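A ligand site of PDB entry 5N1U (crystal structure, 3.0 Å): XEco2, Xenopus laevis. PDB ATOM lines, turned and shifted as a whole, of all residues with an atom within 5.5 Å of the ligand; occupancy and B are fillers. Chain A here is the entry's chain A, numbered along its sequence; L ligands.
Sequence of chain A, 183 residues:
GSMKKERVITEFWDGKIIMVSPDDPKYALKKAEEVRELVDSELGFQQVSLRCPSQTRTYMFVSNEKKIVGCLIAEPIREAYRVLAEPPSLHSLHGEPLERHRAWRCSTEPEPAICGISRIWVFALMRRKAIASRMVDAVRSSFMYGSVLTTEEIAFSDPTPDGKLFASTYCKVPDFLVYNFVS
N of Arg 128 lies within hydrogen-bond range of O11 of the ligand (2.6 Å).
The guanidinium group of Arg 128 lies within salt-bridge range of an oxygen (O3) of the ligand, at 2.5 Å.
The backbone NH of Ser 133 lies within hydrogen-bond range of an oxygen (O8) of the ligand.
O8 of the ligand lies within hydrogen-bond range of OG of Ser 133, at 2.6 Å.
The side-chain hydroxyl (OG1) of Thr 160 is in hydrogen-bond range of a nitrogen (N7) of the ligand (2.8 Å).
An oxygen (O15) of the ligand is in hydrogen-bond range of the backbone NH (N) of Val 122 (3.0 Å).
The backbone NH (N) of Ala 132 sits at hydrogen-bond distance from an oxygen (O12) of the ligand (3.3 Å).
An oxygen (O9) of the ligand lies within hydrogen-bond range of the backbone NH (N) of Ala 130 (3.1 Å).
The side-chain hydroxyl of Thr 169 sits close to an oxygen (O6) of the ligand, at 3.5 Å.
The backbone NH (N) of Lys 129 sits at hydrogen-bond distance from an oxygen (O9) of the ligand (3.5 Å).
O16 of the ligand sits close to O of Ile 120 (2.9 Å).
Residues that only touch the ligand: Arg 127, Gly 163, Leu 165, Phe 166, Trp 121, Leu 43, Ile 131, Asp 162 and Pro 159.
Hydrophobic or aromatic side chains within 4 Å of the ligand: Leu 43, Ile 120, Val 122, Ile 131, Ala 132, Leu 165 and Phe 166.
The side-chain hydroxyl (OG1) of Thr 160 sits at hydrogen-bond distance from the backbone NH (N) of Gly 163.
The side-chain hydroxyl (OG1) of Thr 160 sits close to the backbone NH (N) of Asp 162 (3.5 Å).
O of Val 122 is in hydrogen-bond range of NE of Arg 127, 2.8 Å away.
OG1 of Thr 169 is in hydrogen-bond range of O of Leu 165 (3.2 Å).
O of Lys 129 is in hydrogen-bond range of NH1 of Arg 134.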
ATOM      1  N   LEU A  43      25.552 -25.836 -27.496  1.00  0.00           N
ATOM      2  CA  LEU A  43      25.535 -25.440 -28.903  1.00  0.00           C
ATOM      3  C   LEU A  43      26.289 -26.416 -29.787  1.00  0.00           C
ATOM      4  O   LEU A  43      26.152 -26.348 -31.017  1.00  0.00           O
ATOM      5  CB  LEU A  43      26.134 -24.044 -29.063  1.00  0.00           C
ATOM      6  CG  LEU A  43      25.510 -22.937 -28.209  1.00  0.00           C
ATOM      7  CD1 LEU A  43      26.273 -21.636 -28.391  1.00  0.00           C
ATOM      8  CD2 LEU A  43      24.039 -22.738 -28.552  1.00  0.00           C
ATOM      9  N   ILE A 120      25.064 -17.027 -28.104  1.00  0.00           N
ATOM     10  CA  ILE A 120      24.062 -16.616 -27.123  1.00  0.00           C
ATOM     11  C   ILE A 120      23.261 -17.841 -26.726  1.00  0.00           C
ATOM     12  O   ILE A 120      22.953 -18.687 -27.569  1.00  0.00           O
ATOM     13  CB  ILE A 120      23.143 -15.494 -27.657  1.00  0.00           C
ATOM     14  CG1 ILE A 120      22.033 -15.212 -26.627  1.00  0.00           C
ATOM     15  CG2 ILE A 120      22.556 -15.880 -29.009  1.00  0.00           C
ATOM     16  CD1 ILE A 120      21.182 -14.000 -26.941  1.00  0.00           C
ATOM     17  N   TRP A 121      22.924 -17.929 -25.444  1.00  0.00           N
ATOM     18  CA  TRP A 121      22.239 -19.097 -24.923  1.00  0.00           C
ATOM     19  C   TRP A 121      21.507 -18.709 -23.650  1.00  0.00           C
ATOM     20  O   TRP A 121      22.062 -18.018 -22.795  1.00  0.00           O
ATOM     21  CB  TRP A 121      23.216 -20.241 -24.637  1.00  0.00           C
ATOM     22  CG  TRP A 121      22.698 -21.256 -23.658  1.00  0.00           C
ATOM     23  CD1 TRP A 121      22.017 -22.407 -23.952  1.00  0.00           C
ATOM     24  CD2 TRP A 121      22.812 -21.215 -22.233  1.00  0.00           C
ATOM     25  NE1 TRP A 121      21.709 -23.080 -22.796  1.00  0.00           N
ATOM     26  CE2 TRP A 121      22.177 -22.357 -21.727  1.00  0.00           C
ATOM     27  CE3 TRP A 121      23.393 -20.306 -21.336  1.00  0.00           C
ATOM     28  CZ2 TRP A 121      22.103 -22.635 -20.356  1.00  0.00           C
ATOM     29  CZ3 TRP A 121      23.312 -20.572 -19.980  1.00  0.00           C
ATOM     30  CH2 TRP A 121      22.681 -21.732 -19.506  1.00  0.00           C
ATOM     31  N   VAL A 122      20.253 -19.140 -23.535  1.00  0.00           N
ATOM     32  CA  VAL A 122      19.454 -18.995 -22.335  1.00  0.00           C
ATOM     33  C   VAL A 122      19.107 -20.388 -21.836  1.00  0.00           C
ATOM     34  O   VAL A 122      18.873 -21.294 -22.639  1.00  0.00           O
ATOM     35  CB  VAL A 122      18.176 -18.167 -22.590  1.00  0.00           C
ATOM     36  CG1 VAL A 122      17.326 -18.079 -21.330  1.00  0.00           C
ATOM     37  CG2 VAL A 122      18.527 -16.781 -23.082  1.00  0.00           C
ATOM     38  N   MET A 126      14.080 -21.332 -18.883  1.00  0.00           N
ATOM     39  CA  MET A 126      13.924 -19.915 -18.590  1.00  0.00           C
ATOM     40  C   MET A 126      13.762 -19.075 -19.857  1.00  0.00           C
ATOM     41  O   MET A 126      13.988 -17.854 -19.823  1.00  0.00           O
ATOM     42  CB  MET A 126      15.133 -19.411 -17.788  1.00  0.00           C
ATOM     43  CG  MET A 126      15.230 -19.985 -16.380  1.00  0.00           C
ATOM     44  SD  MET A 126      14.184 -19.108 -15.202  1.00  0.00           S
ATOM     45  CE  MET A 126      14.962 -17.502 -15.144  1.00  0.00           C
ATOM     46  N   ARG A 127      13.363 -19.689 -20.960  1.00  0.00           N
ATOM     47  CA  ARG A 127      13.304 -19.009 -22.248  1.00  0.00           C
ATOM     48  C   ARG A 127      11.928 -18.406 -22.487  1.00  0.00           C
ATOM     49  O   ARG A 127      10.951 -18.752 -21.829  1.00  0.00           O
ATOM     50  CB  ARG A 127      13.667 -19.969 -23.373  1.00  0.00           C
ATOM     51  CG  ARG A 127      15.081 -20.487 -23.262  1.00  0.00           C
ATOM     52  CD  ARG A 127      15.325 -21.635 -24.227  1.00  0.00           C
ATOM     53  NE  ARG A 127      16.704 -22.102 -24.167  1.00  0.00           N
ATOM     54  CZ  ARG A 127      17.198 -23.046 -24.969  1.00  0.00           C
ATOM     55  NH1 ARG A 127      16.425 -23.597 -25.907  1.00  0.00           N
ATOM     56  NH2 ARG A 127      18.455 -23.425 -24.829  1.00  0.00           N
ATOM     57  N   ARG A 128      11.862 -17.503 -23.457  1.00  0.00           N
ATOM     58  CA  ARG A 128      10.679 -16.671 -23.683  1.00  0.00           C
ATOM     59  C   ARG A 128      10.432 -15.759 -22.486  1.00  0.00           C
ATOM     60  O   ARG A 128       9.283 -15.466 -22.141  1.00  0.00           O
ATOM     61  CB  ARG A 128       9.447 -17.524 -24.001  1.00  0.00           C
ATOM     62  CG  ARG A 128       9.630 -18.482 -25.166  1.00  0.00           C
ATOM     63  CD  ARG A 128       9.930 -17.740 -26.471  1.00  0.00           C
ATOM     64  NE  ARG A 128       8.814 -16.870 -26.852  1.00  0.00           N
ATOM     65  CZ  ARG A 128       7.809 -17.219 -27.654  1.00  0.00           C
ATOM     66  NH1 ARG A 128       7.769 -18.435 -28.188  1.00  0.00           N
ATOM     67  NH2 ARG A 128       6.850 -16.345 -27.935  1.00  0.00           N
ATOM     68  N   LYS A 129      11.518 -15.311 -21.862  1.00  0.00           N
ATOM     69  CA  LYS A 129      11.449 -14.420 -20.711  1.00  0.00           C
ATOM     70  C   LYS A 129      12.355 -13.208 -20.913  1.00  0.00           C
ATOM     71  O   LYS A 129      12.781 -12.587 -19.930  1.00  0.00           O
ATOM     72  CB  LYS A 129      11.835 -15.182 -19.440  1.00  0.00           C
ATOM     73  CG  LYS A 129      11.069 -16.488 -19.304  1.00  0.00           C
ATOM     74  CD  LYS A 129      11.414 -17.234 -18.027  1.00  0.00           C
ATOM     75  CE  LYS A 129      10.671 -16.669 -16.818  1.00  0.00           C
ATOM     76  NZ  LYS A 129       9.207 -16.533 -17.035  1.00  0.00           N
ATOM     77  N   ALA A 130      12.645 -12.859 -22.167  1.00  0.00           N
ATOM     78  CA  ALA A 130      13.398 -11.665 -22.526  1.00  0.00           C
ATOM     79  C   ALA A 130      14.809 -11.657 -21.939  1.00  0.00           C
ATOM     80  O   ALA A 130      15.461 -10.616 -21.916  1.00  0.00           O
ATOM     81  CB  ALA A 130      12.661 -10.388 -22.108  1.00  0.00           C
ATOM     82  N   ILE A 131      15.312 -12.816 -21.496  1.00  0.00           N
ATOM     83  CA  ILE A 131      16.684 -12.871 -21.019  1.00  0.00           C
ATOM     84  C   ILE A 131      17.644 -12.596 -22.162  1.00  0.00           C
ATOM     85  O   ILE A 131      18.531 -11.739 -22.060  1.00  0.00           O
ATOM     86  CB  ILE A 131      16.969 -14.223 -20.344  1.00  0.00           C
ATOM     87  CG1 ILE A 131      16.374 -14.232 -18.938  1.00  0.00           C
ATOM     88  CG2 ILE A 131      18.465 -14.512 -20.281  1.00  0.00           C
ATOM     89  CD1 ILE A 131      16.276 -15.597 -18.319  1.00  0.00           C
ATOM     90  N   ALA A 132      17.481 -13.305 -23.279  1.00  0.00           N
ATOM     91  CA  ALA A 132      18.285 -13.027 -24.459  1.00  0.00           C
ATOM     92  C   ALA A 132      18.156 -11.558 -24.860  1.00  0.00           C
ATOM     93  O   ALA A 132      19.161 -10.876 -25.086  1.00  0.00           O
ATOM     94  CB  ALA A 132      17.874 -13.939 -25.610  1.00  0.00           C
ATOM     95  N   SER A 133      16.923 -11.073 -24.945  1.00  0.00           N
ATOM     96  CA  SER A 133      16.707  -9.679 -25.329  1.00  0.00           C
ATOM     97  C   SER A 133      17.467  -8.727 -24.423  1.00  0.00           C
ATOM     98  O   SER A 133      18.113  -7.789 -24.903  1.00  0.00           O
ATOM     99  CB  SER A 133      15.213  -9.373 -25.307  1.00  0.00           C
ATOM    100  OG  SER A 133      14.545  -9.964 -26.404  1.00  0.00           O
ATOM    101  N   ARG A 134      17.411  -8.962 -23.108  1.00  0.00           N
ATOM    102  CA  ARG A 134      18.052  -8.033 -22.165  1.00  0.00           C
ATOM    103  C   ARG A 134      19.571  -8.129 -22.210  1.00  0.00           C
ATOM    104  O   ARG A 134      20.251  -7.126 -21.962  1.00  0.00           O
ATOM    105  CB  ARG A 134      17.533  -8.299 -20.755  1.00  0.00           C
ATOM    106  CG  ARG A 134      16.213  -7.584 -20.462  1.00  0.00           C
ATOM    107  CD  ARG A 134      15.196  -8.516 -19.827  1.00  0.00           C
ATOM    108  NE  ARG A 134      15.265  -8.529 -18.371  1.00  0.00           N
ATOM    109  CZ  ARG A 134      14.781  -9.498 -17.610  1.00  0.00           C
ATOM    110  NH1 ARG A 134      14.189 -10.557 -18.151  1.00  0.00           N
ATOM    111  NH2 ARG A 134      14.891  -9.414 -16.302  1.00  0.00           N
ATOM    112  N   PHE A 156      24.977 -11.433 -35.757  1.00  0.00           N
ATOM    113  CA  PHE A 156      24.974 -12.713 -35.079  1.00  0.00           C
ATOM    114  C   PHE A 156      25.854 -13.700 -35.876  1.00  0.00           C
ATOM    115  O   PHE A 156      25.751 -13.693 -37.077  1.00  0.00           O
ATOM    116  CB  PHE A 156      23.566 -13.296 -34.870  1.00  0.00           C
ATOM    117  CG  PHE A 156      22.649 -12.338 -34.138  1.00  0.00           C
ATOM    118  CD1 PHE A 156      22.403 -11.094 -34.642  1.00  0.00           C
ATOM    119  CD2 PHE A 156      22.040 -12.684 -32.927  1.00  0.00           C
ATOM    120  CE1 PHE A 156      21.577 -10.229 -33.982  1.00  0.00           C
ATOM    121  CE2 PHE A 156      21.231 -11.806 -32.278  1.00  0.00           C
ATOM    122  CZ  PHE A 156      20.996 -10.579 -32.802  1.00  0.00           C
ATOM    123  N   SER A 157      26.622 -14.601 -35.228  1.00  0.00           N
ATOM    124  CA  SER A 157      27.565 -15.524 -35.897  1.00  0.00           C
ATOM    125  C   SER A 157      26.780 -16.796 -36.137  1.00  0.00           C
ATOM    126  O   SER A 157      26.258 -17.271 -35.170  1.00  0.00           O
ATOM    127  CB  SER A 157      28.798 -15.918 -35.044  1.00  0.00           C
ATOM    128  OG  SER A 157      29.390 -17.100 -35.507  1.00  0.00           O
ATOM    129  N   ASP A 158      26.700 -17.313 -37.378  1.00  0.00           N
ATOM    130  CA  ASP A 158      26.048 -18.576 -37.773  1.00  0.00           C
ATOM    131  C   ASP A 158      24.862 -18.961 -36.906  1.00  0.00           C
ATOM    132  O   ASP A 158      24.876 -19.963 -36.229  1.00  0.00           O
ATOM    133  CB  ASP A 158      27.067 -19.737 -37.808  1.00  0.00           C
ATOM    134  CG  ASP A 158      26.445 -21.041 -38.311  1.00  0.00           C
ATOM    135  OD1 ASP A 158      27.105 -22.101 -38.412  1.00  0.00           O
ATOM    136  OD2 ASP A 158      25.259 -21.006 -38.653  1.00  0.00           O
ATOM    137  N   PRO A 159      23.841 -18.116 -36.898  1.00  0.00           N
ATOM    138  CA  PRO A 159      22.696 -18.331 -36.041  1.00  0.00           C
ATOM    139  C   PRO A 159      21.978 -19.616 -36.324  1.00  0.00           C
ATOM    140  O   PRO A 159      21.863 -19.985 -37.458  1.00  0.00           O
ATOM    141  CB  PRO A 159      21.830 -17.111 -36.341  1.00  0.00           C
ATOM    142  CG  PRO A 159      22.087 -16.889 -37.765  1.00  0.00           C
ATOM    143  CD  PRO A 159      23.481 -17.283 -38.047  1.00  0.00           C
ATOM    144  N   THR A 160      21.527 -20.289 -35.284  1.00  0.00           N
ATOM    145  CA  THR A 160      20.744 -21.504 -35.401  1.00  0.00           C
ATOM    146  C   THR A 160      19.302 -21.095 -35.654  1.00  0.00           C
ATOM    147  O   THR A 160      18.957 -19.914 -35.554  1.00  0.00           O
ATOM    148  CB  THR A 160      20.873 -22.343 -34.133  1.00  0.00           C
ATOM    149  OG1 THR A 160      19.852 -21.966 -33.203  1.00  0.00           O
ATOM    150  CG2 THR A 160      22.245 -22.176 -33.471  1.00  0.00           C
ATOM    151  N   ASP A 162      16.481 -21.325 -33.892  1.00  0.00           N
ATOM    152  CA  ASP A 162      16.042 -20.528 -32.762  1.00  0.00           C
ATOM    153  C   ASP A 162      16.645 -19.133 -32.811  1.00  0.00           C
ATOM    154  O   ASP A 162      15.928 -18.126 -32.745  1.00  0.00           O
ATOM    155  CB  ASP A 162      16.434 -21.220 -31.446  1.00  0.00           C
ATOM    156  CG  ASP A 162      15.535 -22.398 -31.130  1.00  0.00           C
ATOM    157  OD1 ASP A 162      15.626 -22.911 -29.993  1.00  0.00           O
ATOM    158  OD2 ASP A 162      14.740 -22.791 -32.002  1.00  0.00           O
ATOM    159  N   GLY A 163      17.970 -19.045 -32.941  1.00  0.00           N
ATOM    160  CA  GLY A 163      18.614 -17.743 -33.049  1.00  0.00           C
ATOM    161  C   GLY A 163      17.991 -16.887 -34.137  1.00  0.00           C
ATOM    162  O   GLY A 163      17.666 -15.721 -33.916  1.00  0.00           O
ATOM    163  N   LYS A 164      17.820 -17.463 -35.330  1.00  0.00           N
ATOM    164  CA  LYS A 164      17.178 -16.728 -36.418  1.00  0.00           C
ATOM    165  C   LYS A 164      15.786 -16.249 -36.018  1.00  0.00           C
ATOM    166  O   LYS A 164      15.392 -15.118 -36.339  1.00  0.00           O
ATOM    167  CB  LYS A 164      17.132 -17.597 -37.678  1.00  0.00           C
ATOM    168  CG  LYS A 164      16.644 -16.874 -38.921  1.00  0.00           C
ATOM    169  CD  LYS A 164      16.634 -17.794 -40.130  1.00  0.00           C
ATOM    170  CE  LYS A 164      16.127 -17.079 -41.387  1.00  0.00           C
ATOM    171  NZ  LYS A 164      14.679 -16.761 -41.261  1.00  0.00           N
ATOM    172  N   LEU A 165      15.024 -17.090 -35.322  1.00  0.00           N
ATOM    173  CA  LEU A 165      13.716 -16.664 -34.824  1.00  0.00           C
ATOM    174  C   LEU A 165      13.853 -15.539 -33.806  1.00  0.00           C
ATOM    175  O   LEU A 165      12.948 -14.708 -33.666  1.00  0.00           O
ATOM    176  CB  LEU A 165      12.967 -17.842 -34.210  1.00  0.00           C
ATOM    177  CG  LEU A 165      12.189 -18.744 -35.177  1.00  0.00           C
ATOM    178  CD1 LEU A 165      13.119 -19.665 -35.953  1.00  0.00           C
ATOM    179  CD2 LEU A 165      11.137 -19.543 -34.433  1.00  0.00           C
ATOM    180  N   PHE A 166      14.977 -15.486 -33.083  1.00  0.00           N
ATOM    181  CA  PHE A 166      15.185 -14.454 -32.069  1.00  0.00           C
ATOM    182  C   PHE A 166      15.621 -13.134 -32.691  1.00  0.00           C
ATOM    183  O   PHE A 166      15.076 -12.077 -32.377  1.00  0.00           O
ATOM    184  CB  PHE A 166      16.210 -14.927 -31.044  1.00  0.00           C
ATOM    185  CG  PHE A 166      16.740 -13.834 -30.158  1.00  0.00           C
ATOM    186  CD1 PHE A 166      16.068 -13.481 -29.003  1.00  0.00           C
ATOM    187  CD2 PHE A 166      17.906 -13.164 -30.487  1.00  0.00           C
ATOM    188  CE1 PHE A 166      16.551 -12.468 -28.194  1.00  0.00           C
ATOM    189  CE2 PHE A 166      18.389 -12.166 -29.677  1.00  0.00           C
ATOM    190  CZ  PHE A 166      17.722 -11.807 -28.533  1.00  0.00           C
ATOM    191  N   THR A 169      12.999 -11.014 -34.579  1.00  0.00           N
ATOM    192  CA  THR A 169      12.107 -10.221 -33.737  1.00  0.00           C
ATOM    193  C   THR A 169      12.862  -9.088 -33.051  1.00  0.00           C
ATOM    194  O   THR A 169      12.372  -7.949 -33.004  1.00  0.00           O
ATOM    195  CB  THR A 169      11.444 -11.119 -32.683  1.00  0.00           C
ATOM    196  OG1 THR A 169      10.925 -12.295 -33.307  1.00  0.00           O
ATOM    197  CG2 THR A 169      10.313 -10.366 -32.004  1.00  0.00           C
ATOM    198  N   TYR A 170      14.042  -9.368 -32.499  1.00  0.00           N
ATOM    199  CA  TYR A 170      14.790  -8.351 -31.771  1.00  0.00           C
ATOM    200  C   TYR A 170      15.204  -7.207 -32.684  1.00  0.00           C
ATOM    201  O   TYR A 170      14.974  -6.030 -32.371  1.00  0.00           O
ATOM    202  CB  TYR A 170      16.027  -8.975 -31.112  1.00  0.00           C
ATOM    203  CG  TYR A 170      16.838  -7.973 -30.329  1.00  0.00           C
ATOM    204  CD1 TYR A 170      16.401  -7.525 -29.087  1.00  0.00           C
ATOM    205  CD2 TYR A 170      18.025  -7.452 -30.831  1.00  0.00           C
ATOM    206  CE1 TYR A 170      17.125  -6.595 -28.369  1.00  0.00           C
ATOM    207  CE2 TYR A 170      18.749  -6.522 -30.113  1.00  0.00           C
ATOM    208  CZ  TYR A 170      18.302  -6.097 -28.887  1.00  0.00           C
ATOM    209  OH  TYR A 170      19.015  -5.174 -28.170  1.00  0.00           O
HETATM  210  N1  LIG L   1      10.474 -19.366 -31.154  1.00  0.00           N
HETATM  211  C1  LIG L   1       9.635 -18.401 -31.625  1.00  0.00           C
HETATM  212  N2  LIG L   1       9.871 -17.076 -31.375  1.00  0.00           N
HETATM  213  C2  LIG L   1      10.948 -16.720 -30.629  1.00  0.00           C
HETATM  214  C3  LIG L   1      11.767 -17.663 -30.157  1.00  0.00           C
HETATM  215  C4  LIG L   1      11.529 -19.012 -30.429  1.00  0.00           C
HETATM  216  N3  LIG L   1      12.272 -20.170 -30.028  1.00  0.00           N
HETATM  217  N4  LIG L   1      12.744 -17.064 -29.458  1.00  0.00           N
HETATM  218  C5  LIG L   1      12.537 -15.743 -29.499  1.00  0.00           C
HETATM  219  N5  LIG L   1      11.429 -15.518 -30.206  1.00  0.00           N
HETATM  220  C6  LIG L   1      10.845 -14.233 -30.498  1.00  0.00           C
HETATM  221  C7  LIG L   1       9.789 -13.991 -29.744  1.00  0.00           C
HETATM  222  O1  LIG L   1       8.947 -13.009 -30.369  1.00  0.00           O
HETATM  223  C8  LIG L   1      10.414 -13.398 -28.453  1.00  0.00           C
HETATM  224  O2  LIG L   1       9.558 -12.624 -27.773  1.00  0.00           O
HETATM  225  P1  LIG L   1       8.062 -13.235 -27.262  1.00  0.00           P
HETATM  226  O3  LIG L   1       8.259 -14.502 -26.467  1.00  0.00           O
HETATM  227  O4  LIG L   1       7.178 -13.529 -28.501  1.00  0.00           O
HETATM  228  O5  LIG L   1       7.383 -12.204 -26.393  1.00  0.00           O
HETATM  229  C9  LIG L   1      11.574 -12.506 -29.008  1.00  0.00           C
HETATM  230  O6  LIG L   1      11.963 -13.094 -30.110  1.00  0.00           O
HETATM  231  C10 LIG L   1      12.709 -12.411 -27.997  1.00  0.00           C
HETATM  232  O7  LIG L   1      12.990 -13.674 -27.468  1.00  0.00           O
HETATM  233  P2  LIG L   1      13.724 -13.772 -25.994  1.00  0.00           P
HETATM  234  O8  LIG L   1      14.264 -12.413 -25.630  1.00  0.00           O
HETATM  235  O9  LIG L   1      12.760 -14.242 -24.940  1.00  0.00           O
HETATM  236  O10 LIG L   1      14.985 -14.849 -26.099  1.00  0.00           O
HETATM  237  P3  LIG L   1      15.113 -16.187 -25.064  1.00  0.00           P
HETATM  238  O11 LIG L   1      13.820 -16.983 -25.145  1.00  0.00           O
HETATM  239  O12 LIG L   1      15.346 -15.734 -23.639  1.00  0.00           O
HETATM  240  O13 LIG L   1      16.371 -17.159 -25.544  1.00  0.00           O
HETATM  241  C11 LIG L   1      15.948 -18.846 -27.231  1.00  0.00           C
HETATM  242  C12 LIG L   1      16.065 -18.535 -25.750  1.00  0.00           C
HETATM  243  C13 LIG L   1      14.962 -17.912 -27.844  1.00  0.00           C
HETATM  244  C14 LIG L   1      15.426 -20.245 -27.454  1.00  0.00           C
HETATM  245  C15 LIG L   1      17.320 -18.642 -27.879  1.00  0.00           C
HETATM  246  O14 LIG L   1      17.723 -17.365 -27.609  1.00  0.00           O
HETATM  247  C16 LIG L   1      18.336 -19.641 -27.266  1.00  0.00           C
HETATM  248  O15 LIG L   1      19.001 -19.328 -26.288  1.00  0.00           O
HETATM  249  N6  LIG L   1      18.486 -21.019 -27.892  1.00  0.00           N
HETATM  250  C17 LIG L   1      19.477 -22.039 -27.344  1.00  0.00           C
HETATM  251  C18 LIG L   1      20.529 -22.305 -28.418  1.00  0.00           C
HETATM  252  C19 LIG L   1      20.637 -21.034 -29.283  1.00  0.00           C
HETATM  253  O16 LIG L   1      20.701 -19.955 -28.771  1.00  0.00           O
HETATM  254  N7  LIG L   1      20.648 -21.107 -30.683  1.00  0.00           N
HETATM  255  C20 LIG L   1      20.736 -19.867 -31.453  1.00  0.00           C
HETATM  256  C21 LIG L   1      22.125 -19.175 -31.226  1.00  0.00           C
HETATM  257  S1  LIG L   1      22.202 -17.706 -32.340  1.00  0.00           S
